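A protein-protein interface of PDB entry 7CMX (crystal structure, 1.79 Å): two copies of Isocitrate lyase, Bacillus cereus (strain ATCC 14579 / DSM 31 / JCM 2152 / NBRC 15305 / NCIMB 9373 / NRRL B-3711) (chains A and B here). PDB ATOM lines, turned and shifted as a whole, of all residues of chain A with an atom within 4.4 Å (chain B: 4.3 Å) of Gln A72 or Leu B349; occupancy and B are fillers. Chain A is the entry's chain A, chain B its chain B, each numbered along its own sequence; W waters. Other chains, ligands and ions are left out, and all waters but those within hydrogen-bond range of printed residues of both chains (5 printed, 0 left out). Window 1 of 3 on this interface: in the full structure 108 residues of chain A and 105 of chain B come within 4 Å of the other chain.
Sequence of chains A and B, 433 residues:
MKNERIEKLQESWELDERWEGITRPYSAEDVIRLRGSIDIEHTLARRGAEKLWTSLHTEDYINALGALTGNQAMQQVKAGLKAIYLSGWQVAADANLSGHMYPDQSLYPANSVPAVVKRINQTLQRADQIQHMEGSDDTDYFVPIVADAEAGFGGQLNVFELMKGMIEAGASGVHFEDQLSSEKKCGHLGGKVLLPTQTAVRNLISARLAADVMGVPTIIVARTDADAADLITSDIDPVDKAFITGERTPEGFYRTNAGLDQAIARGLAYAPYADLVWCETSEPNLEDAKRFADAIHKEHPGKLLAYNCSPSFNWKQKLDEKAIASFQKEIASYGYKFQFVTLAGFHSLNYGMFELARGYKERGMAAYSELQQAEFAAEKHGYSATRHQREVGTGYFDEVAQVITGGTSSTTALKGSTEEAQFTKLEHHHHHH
OD2 of Asp B94 is in hydrogen-bond range of OG1 of Thr A69, 3.0 Å away.
The side-chain carboxylate (OD1) of Asp B94 sits at hydrogen-bond distance from the backbone NH (N) of Gly A70, at 3.3 Å.
N of Asn A71 lies within hydrogen-bond range of OD1 of Asp B94 (2.9 Å).
The side-chain amide nitrogen of Asn B350 sits at hydrogen-bond distance from the side-chain amide oxygen of Asn A71, at 3.0 Å.
NE2 of Gln A75 is in hydrogen-bond range of OD1 of Asn B350, at 2.8 Å.
The side-chain sulfur (SD) of Met B353 sits at hydrogen-bond distance from the side-chain amide nitrogen (NE2) of Gln A76, 3.6 Å away.
Printed residues of chain A that touch a printed residue of chain B: Gly A66, Thr A69, Gly A70, Asn A71, Gln A72, Gln A75, Gln A76, Gly A345 and Leu A349.
Of the 11 printed residues of chain B, 6 touch a printed residue of chain A.
Printed residues of chain B that touch a printed residue of chain A: Gln B72, Asp B94, Phe B346, Leu B349, Asn B350 and Met B353.
Hydrophobic or aromatic side chains of chain B that line the printed part of chain A: Phe B346, Leu B349 and Met B353.
Along chain B the printed residues that touch a printed residue of chain A span positions 72 to 353.
Among the printed residues, 14 pairs touch across the chains.
Among the printed residues, no Asp or Glu carboxylate lies within 4 Å of a Lys or Arg side-chain nitrogen of the other chain.
Among the printed residues, pairs that only touch across the chains: Asn A71 with Phe B346 (3.2 Å), Gln A72 with Met B353 (3.3 Å), Asn A71 with Leu B349 (3.6 Å), Gln A72 with Leu B349 (3.6 Å), Gly A345 with Met B353 (3.7 Å), Leu A349 with Gln B72 (3.7 Å), Thr A69 with Leu B349 (3.9 Å) and Gly A66 with Met B353 (3.97 Å).
Water W1 lies within hydrogen-bond range of OD1 of Asn A71 (2.5 Å) and OD2 of Asp B94 (2.8 Å).
Water W4 lies within hydrogen-bond range of the side-chain carboxylate of Asp B94 (2.7 Å) and the side-chain amide nitrogen of Asn A71 (3.3 Å).
Water W3 lies within hydrogen-bond range of the backbone carbonyl oxygen of Leu A349 (2.7 Å), the side-chain hydroxyl of Ser B348 (2.9 Å) and the side-chain amide nitrogen of Gln B72 (3.0 Å).
Water W2 bridges OD1 of Asp B94 (2.8 Å) and N of Gly A70 (3.0 Å).
Water W5 lies within hydrogen-bond range of O of Leu B349 (2.8 Å) and NE2 of Gln A72 (3.1 Å).
NE2 of Gln A76 lies within hydrogen-bond range of O of Gly A66 (3.1 Å).
N of Leu A68 lies close to OE1 of Gln A72.
The backbone NH (N) of Asn A71 lies close to the side-chain hydroxyl (OG1) of Thr A69 (3.5 Å).
NE2 of Gln A72 sits at hydrogen-bond distance from O of Gly A345 (3.1 Å).
NE2 of Gln B72 sits at hydrogen-bond distance from O of Gly B345 (3.2 Å).
The side-chain amide nitrogen of Asn B350 sits at hydrogen-bond distance from the backbone carbonyl oxygen of Phe B346 (2.9 Å).
Of chain B, only Leu B349 (3.6 Å) and Met B353 (3.3 Å) come within 4 Å of Gln A72.
Of the printed residues of chain B, Gly A70 touches Asp B94 (3.3 Å).
Printed residues of chain B within 4 Å of Gly A66: Met B353.
Of the printed residues of chain A, Phe B346 touches Asn A71 (3.2 Å).
Printed residues of chain A within 4 Å of Met B353: Gly A66, Gln A72, Gln A76 and Gly A345.
Of the printed residues of chain B, Asn A71 touches Asp B94 (2.9 Å), Phe B346 (3.2 Å), Leu B349 (3.6 Å) and Asn B350 (3.0 Å).
The nearest residue of chain A that does not touch Leu B349 is Leu A349 (4.1 Å).
The nearest printed residue of chain B that does not touch Gly A345 is Leu B349 (6.9 Å).
Gln A72 touches Leu B349, and with the chains exchanged Leu A349 touches Gln B72.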
ATOM      1  N   GLY A  66      -2.169  -1.758  -5.855  1.00  0.00           N
ATOM      2  CA  GLY A  66      -3.075  -1.283  -4.788  1.00  0.00           C
ATOM      3  C   GLY A  66      -4.526  -1.377  -5.218  1.00  0.00           C
ATOM      4  O   GLY A  66      -4.842  -1.058  -6.390  1.00  0.00           O
ATOM      5  N   ALA A  67      -5.384  -1.915  -4.367  1.00  0.00           N
ATOM      6  CA  ALA A  67      -6.837  -1.963  -4.626  1.00  0.00           C
ATOM      7  C   ALA A  67      -7.547  -1.303  -3.450  1.00  0.00           C
ATOM      8  O   ALA A  67      -7.187  -1.676  -2.328  1.00  0.00           O
ATOM      9  CB  ALA A  67      -7.284  -3.381  -4.805  1.00  0.00           C
ATOM     10  N   LEU A  68      -8.503  -0.402  -3.690  1.00  0.00           N
ATOM     11  CA  LEU A  68      -9.274   0.196  -2.570  1.00  0.00           C
ATOM     12  C   LEU A  68     -10.740  -0.243  -2.589  1.00  0.00           C
ATOM     13  O   LEU A  68     -11.470   0.166  -1.653  1.00  0.00           O
ATOM     14  CB  LEU A  68      -9.073   1.719  -2.433  1.00  0.00           C
ATOM     15  CG  LEU A  68      -9.408   2.759  -3.513  1.00  0.00           C
ATOM     16  CD1 LEU A  68      -8.859   2.475  -4.880  1.00  0.00           C
ATOM     17  CD2 LEU A  68     -10.873   3.188  -3.556  1.00  0.00           C
ATOM     18  N   THR A  69     -11.130  -1.093  -3.537  1.00  0.00           N
ATOM     19  CA  THR A  69     -12.490  -1.684  -3.645  1.00  0.00           C
ATOM     20  C   THR A  69     -12.363  -3.122  -4.128  1.00  0.00           C
ATOM     21  O   THR A  69     -11.398  -3.402  -4.872  1.00  0.00           O
ATOM     22  CB  THR A  69     -13.412  -0.948  -4.632  1.00  0.00           C
ATOM     23  OG1 THR A  69     -13.108  -1.315  -5.982  1.00  0.00           O
ATOM     24  CG2 THR A  69     -13.370   0.553  -4.491  1.00  0.00           C
ATOM     25  N   GLY A  70     -13.319  -3.976  -3.745  1.00  0.00           N
ATOM     26  CA  GLY A  70     -13.445  -5.357  -4.261  1.00  0.00           C
ATOM     27  C   GLY A  70     -13.431  -5.417  -5.785  1.00  0.00           C
ATOM     28  O   GLY A  70     -12.741  -6.290  -6.346  1.00  0.00           O
ATOM     29  N   ASN A  71     -14.186  -4.560  -6.458  1.00  0.00           N
ATOM     30  CA  ASN A  71     -14.240  -4.584  -7.941  1.00  0.00           C
ATOM     31  C   ASN A  71     -12.832  -4.376  -8.533  1.00  0.00           C
ATOM     32  O   ASN A  71     -12.517  -5.068  -9.491  1.00  0.00           O
ATOM     33  CB  ASN A  71     -15.175  -3.528  -8.502  1.00  0.00           C
ATOM     34  CG  ASN A  71     -16.634  -3.912  -8.477  1.00  0.00           C
ATOM     35  OD1 ASN A  71     -17.432  -3.154  -9.016  1.00  0.00           O
ATOM     36  ND2 ASN A  71     -16.999  -5.033  -7.861  1.00  0.00           N
ATOM     37  N   GLN A  72     -12.025  -3.462  -7.985  1.00  0.00           N
ATOM     38  CA  GLN A  72     -10.631  -3.247  -8.458  1.00  0.00           C
ATOM     39  C   GLN A  72      -9.835  -4.539  -8.270  1.00  0.00           C
ATOM     40  O   GLN A  72      -9.096  -4.910  -9.199  1.00  0.00           O
ATOM     41  CB  GLN A  72      -9.952  -2.101  -7.717  1.00  0.00           C
ATOM     42  CG  GLN A  72     -10.408  -0.734  -8.178  1.00  0.00           C
ATOM     43  CD  GLN A  72      -9.546   0.370  -7.610  1.00  0.00           C
ATOM     44  OE1 GLN A  72      -9.017   0.250  -6.509  1.00  0.00           O
ATOM     45  NE2 GLN A  72      -9.371   1.427  -8.387  1.00  0.00           N
ATOM     46  N   ALA A  73      -9.948  -5.176  -7.101  1.00  0.00           N
ATOM     47  CA  ALA A  73      -9.254  -6.450  -6.796  1.00  0.00           C
ATOM     48  C   ALA A  73      -9.739  -7.556  -7.756  1.00  0.00           C
ATOM     49  O   ALA A  73      -8.894  -8.316  -8.314  1.00  0.00           O
ATOM     50  CB  ALA A  73      -9.520  -6.823  -5.359  1.00  0.00           C
ATOM     51  N   MET A  74     -11.049  -7.667  -7.950  1.00  0.00           N
ATOM     52  CA  MET A  74     -11.642  -8.654  -8.896  1.00  0.00           C
ATOM     53  C   MET A  74     -11.034  -8.484 -10.314  1.00  0.00           C
ATOM     54  O   MET A  74     -10.640  -9.509 -10.918  1.00  0.00           O
ATOM     55  CB  MET A  74     -13.158  -8.484  -8.928  1.00  0.00           C
ATOM     56  CG  MET A  74     -13.872  -9.397  -9.872  1.00  0.00           C
ATOM     57  SD  MET A  74     -15.660  -9.337  -9.563  1.00  0.00           S
ATOM     58  CE  MET A  74     -15.999  -7.604  -9.846  1.00  0.00           C
ATOM     59  N   GLN A  75     -10.880  -7.254 -10.824  1.00  0.00           N
ATOM     60  CA  GLN A  75     -10.314  -7.041 -12.191  1.00  0.00           C
ATOM     61  C   GLN A  75      -8.819  -7.404 -12.201  1.00  0.00           C
ATOM     62  O   GLN A  75      -8.302  -7.878 -13.250  1.00  0.00           O
ATOM     63  CB  GLN A  75     -10.540  -5.602 -12.674  1.00  0.00           C
ATOM     64  CG  GLN A  75     -12.010  -5.219 -12.812  1.00  0.00           C
ATOM     65  CD  GLN A  75     -12.890  -6.183 -13.569  1.00  0.00           C
ATOM     66  OE1 GLN A  75     -12.452  -6.842 -14.512  1.00  0.00           O
ATOM     67  NE2 GLN A  75     -14.161  -6.257 -13.174  1.00  0.00           N
ATOM     68  N   GLN A  76      -8.113  -7.144 -11.094  1.00  0.00           N
ATOM     69  CA  GLN A  76      -6.677  -7.470 -10.960  1.00  0.00           C
ATOM     70  C   GLN A  76      -6.523  -8.990 -11.118  1.00  0.00           C
ATOM     71  O   GLN A  76      -5.620  -9.416 -11.858  1.00  0.00           O
ATOM     72  CB  GLN A  76      -6.133  -6.932  -9.635  1.00  0.00           C
ATOM     73  CG  GLN A  76      -5.968  -5.420  -9.600  1.00  0.00           C
ATOM     74  CD  GLN A  76      -5.666  -4.888  -8.218  1.00  0.00           C
ATOM     75  OE1 GLN A  76      -5.507  -5.646  -7.299  1.00  0.00           O
ATOM     76  NE2 GLN A  76      -5.543  -3.579  -8.072  1.00  0.00           N
ATOM     77  N   GLY A 345      -4.537   1.947  -7.496  1.00  0.00           N
ATOM     78  CA  GLY A 345      -5.999   2.035  -7.409  1.00  0.00           C
ATOM     79  C   GLY A 345      -6.445   3.483  -7.388  1.00  0.00           C
ATOM     80  O   GLY A 345      -7.410   3.822  -8.077  1.00  0.00           O
ATOM     81  N   LEU A 349      -8.572   5.037 -10.523  1.00  0.00           N
ATOM     82  CA  LEU A 349      -9.957   5.514 -10.238  1.00  0.00           C
ATOM     83  C   LEU A 349     -10.048   7.009 -10.559  1.00  0.00           C
ATOM     84  O   LEU A 349     -11.008   7.402 -11.261  1.00  0.00           O
ATOM     85  CB  LEU A 349     -10.312   5.224  -8.775  1.00  0.00           C
ATOM     86  CG  LEU A 349     -11.645   5.752  -8.249  1.00  0.00           C
ATOM     87  CD1 LEU A 349     -12.101   4.940  -7.030  1.00  0.00           C
ATOM     88  CD2 LEU A 349     -11.541   7.220  -7.864  1.00  0.00           C
ATOM     89  N   GLN B  72     -14.211   9.868  -7.032  1.00  0.00           N
ATOM     90  CA  GLN B  72     -14.919   9.911  -8.334  1.00  0.00           C
ATOM     91  C   GLN B  72     -15.708  11.219  -8.456  1.00  0.00           C
ATOM     92  O   GLN B  72     -15.669  11.873  -9.521  1.00  0.00           O
ATOM     93  CB  GLN B  72     -15.840   8.710  -8.479  1.00  0.00           C
ATOM     94  CG  GLN B  72     -15.083   7.455  -8.849  1.00  0.00           C
ATOM     95  CD  GLN B  72     -15.996   6.327  -9.261  1.00  0.00           C
ATOM     96  OE1 GLN B  72     -17.120   6.238  -8.795  1.00  0.00           O
ATOM     97  NE2 GLN B  72     -15.520   5.456 -10.125  1.00  0.00           N
ATOM     98  N   ASP B  94     -20.484  -2.644  -4.858  1.00  0.00           N
ATOM     99  CA  ASP B  94     -19.081  -2.351  -4.453  1.00  0.00           C
ATOM    100  C   ASP B  94     -18.953  -1.338  -3.312  1.00  0.00           C
ATOM    101  O   ASP B  94     -17.813  -1.012  -3.006  1.00  0.00           O
ATOM    102  CB  ASP B  94     -18.299  -1.826  -5.665  1.00  0.00           C
ATOM    103  CG  ASP B  94     -16.781  -2.028  -5.666  1.00  0.00           C
ATOM    104  OD1 ASP B  94     -16.251  -3.046  -5.042  1.00  0.00           O
ATOM    105  OD2 ASP B  94     -16.113  -1.176  -6.309  1.00  0.00           O
ATOM    106  N   GLY B 345     -19.701   5.147 -12.808  1.00  0.00           N
ATOM    107  CA  GLY B 345     -18.677   4.893 -11.786  1.00  0.00           C
ATOM    108  C   GLY B 345     -18.187   3.452 -11.850  1.00  0.00           C
ATOM    109  O   GLY B 345     -17.005   3.228 -11.857  1.00  0.00           O
ATOM    110  N   PHE B 346     -19.091   2.503 -11.938  1.00  0.00           N
ATOM    111  CA  PHE B 346     -18.773   1.054 -12.053  1.00  0.00           C
ATOM    112  C   PHE B 346     -17.916   0.810 -13.302  1.00  0.00           C
ATOM    113  O   PHE B 346     -16.889   0.144 -13.216  1.00  0.00           O
ATOM    114  CB  PHE B 346     -20.064   0.242 -12.036  1.00  0.00           C
ATOM    115  CG  PHE B 346     -19.874  -1.231 -12.279  1.00  0.00           C
ATOM    116  CD1 PHE B 346     -19.867  -1.751 -13.563  1.00  0.00           C
ATOM    117  CD2 PHE B 346     -19.737  -2.101 -11.220  1.00  0.00           C
ATOM    118  CE1 PHE B 346     -19.725  -3.122 -13.779  1.00  0.00           C
ATOM    119  CE2 PHE B 346     -19.544  -3.459 -11.436  1.00  0.00           C
ATOM    120  CZ  PHE B 346     -19.571  -3.977 -12.710  1.00  0.00           C
ATOM    121  N   HIS B 347     -18.326   1.312 -14.465  1.00  0.00           N
ATOM    122  CA  HIS B 347     -17.675   0.919 -15.742  1.00  0.00           C
ATOM    123  C   HIS B 347     -16.300   1.581 -15.826  1.00  0.00           C
ATOM    124  O   HIS B 347     -15.363   0.919 -16.296  1.00  0.00           O
ATOM    125  CB  HIS B 347     -18.578   1.224 -16.945  1.00  0.00           C
ATOM    126  CG  HIS B 347     -19.665   0.214 -17.054  1.00  0.00           C
ATOM    127  ND1 HIS B 347     -19.423  -1.064 -17.546  1.00  0.00           N
ATOM    128  CD2 HIS B 347     -20.964   0.265 -16.707  1.00  0.00           C
ATOM    129  CE1 HIS B 347     -20.563  -1.740 -17.513  1.00  0.00           C
ATOM    130  NE2 HIS B 347     -21.509  -0.954 -16.991  1.00  0.00           N
ATOM    131  N   SER B 348     -16.194   2.841 -15.395  1.00  0.00           N
ATOM    132  CA  SER B 348     -14.912   3.583 -15.320  1.00  0.00           C
ATOM    133  C   SER B 348     -13.938   2.810 -14.420  1.00  0.00           C
ATOM    134  O   SER B 348     -12.738   2.627 -14.803  1.00  0.00           O
ATOM    135  CB  SER B 348     -15.170   5.000 -14.807  1.00  0.00           C
ATOM    136  OG  SER B 348     -13.964   5.701 -14.611  1.00  0.00           O
ATOM    137  N   LEU B 349     -14.412   2.397 -13.236  1.00  0.00           N
ATOM    138  CA  LEU B 349     -13.549   1.806 -12.188  1.00  0.00           C
ATOM    139  C   LEU B 349     -13.068   0.446 -12.700  1.00  0.00           C
ATOM    140  O   LEU B 349     -11.846   0.200 -12.654  1.00  0.00           O
ATOM    141  CB  LEU B 349     -14.335   1.669 -10.878  1.00  0.00           C
ATOM    142  CG  LEU B 349     -13.551   1.064  -9.718  1.00  0.00           C
ATOM    143  CD1 LEU B 349     -13.999   1.618  -8.371  1.00  0.00           C
ATOM    144  CD2 LEU B 349     -13.696  -0.440  -9.703  1.00  0.00           C
ATOM    145  N   ASN B 350     -13.995  -0.372 -13.209  1.00  0.00           N
ATOM    146  CA  ASN B 350     -13.731  -1.777 -13.602  1.00  0.00           C
ATOM    147  C   ASN B 350     -12.894  -1.774 -14.875  1.00  0.00           C
ATOM    148  O   ASN B 350     -11.914  -2.525 -14.915  1.00  0.00           O
ATOM    149  CB  ASN B 350     -15.020  -2.603 -13.696  1.00  0.00           C
ATOM    150  CG  ASN B 350     -15.503  -3.050 -12.334  1.00  0.00           C
ATOM    151  OD1 ASN B 350     -14.962  -4.003 -11.766  1.00  0.00           O
ATOM    152  ND2 ASN B 350     -16.441  -2.321 -11.746  1.00  0.00           N
ATOM    153  N   TYR B 351     -13.267  -0.986 -15.895  1.00  0.00           N
ATOM    154  CA  TYR B 351     -12.538  -0.995 -17.181  1.00  0.00           C
ATOM    155  C   TYR B 351     -11.100  -0.532 -16.926  1.00  0.00           C
ATOM    156  O   TYR B 351     -10.153  -1.177 -17.430  1.00  0.00           O
ATOM    157  CB  TYR B 351     -13.175  -0.094 -18.242  1.00  0.00           C
ATOM    158  CG  TYR B 351     -12.370  -0.050 -19.514  1.00  0.00           C
ATOM    159  CD1 TYR B 351     -12.303  -1.161 -20.343  1.00  0.00           C
ATOM    160  CD2 TYR B 351     -11.618   1.069 -19.860  1.00  0.00           C
ATOM    161  CE1 TYR B 351     -11.555  -1.143 -21.512  1.00  0.00           C
ATOM    162  CE2 TYR B 351     -10.856   1.097 -21.015  1.00  0.00           C
ATOM    163  CZ  TYR B 351     -10.846  -0.008 -21.849  1.00  0.00           C
ATOM    164  OH  TYR B 351     -10.086  -0.004 -22.983  1.00  0.00           O
ATOM    165  N   GLY B 352     -10.951   0.585 -16.207  1.00  0.00           N
ATOM    166  CA  GLY B 352      -9.634   1.210 -15.983  1.00  0.00           C
ATOM    167  C   GLY B 352      -8.669   0.263 -15.282  1.00  0.00           C
ATOM    168  O   GLY B 352      -7.492   0.189 -15.677  1.00  0.00           O
ATOM    169  N   MET B 353      -9.115  -0.387 -14.222  1.00  0.00           N
ATOM    170  CA  MET B 353      -8.253  -1.289 -13.415  1.00  0.00           C
ATOM    171  C   MET B 353      -7.978  -2.566 -14.220  1.00  0.00           C
ATOM    172  O   MET B 353      -6.879  -3.056 -14.130  1.00  0.00           O
ATOM    173  CB  MET B 353      -8.906  -1.657 -12.076  1.00  0.00           C
ATOM    174  CG  MET B 353      -8.011  -2.537 -11.207  1.00  0.00           C
ATOM    175  SD  MET B 353      -6.317  -1.868 -11.136  1.00  0.00           S
ATOM    176  CE  MET B 353      -6.538  -0.544  -9.940  1.00  0.00           C
HETATM  177  O   HOH W   1     -17.422  -0.623  -8.723  1.00  0.00           O
HETATM  178  O   HOH W   2     -15.686  -2.799  -2.337  1.00  0.00           O
HETATM  179  O   HOH W   3     -13.081   5.705 -11.869  1.00  0.00           O
HETATM  180  O   HOH W   4     -17.529  -5.395  -4.597  1.00  0.00           O
HETATM  181  O   HOH W   5     -10.118   1.925 -11.303  1.00  0.00           O
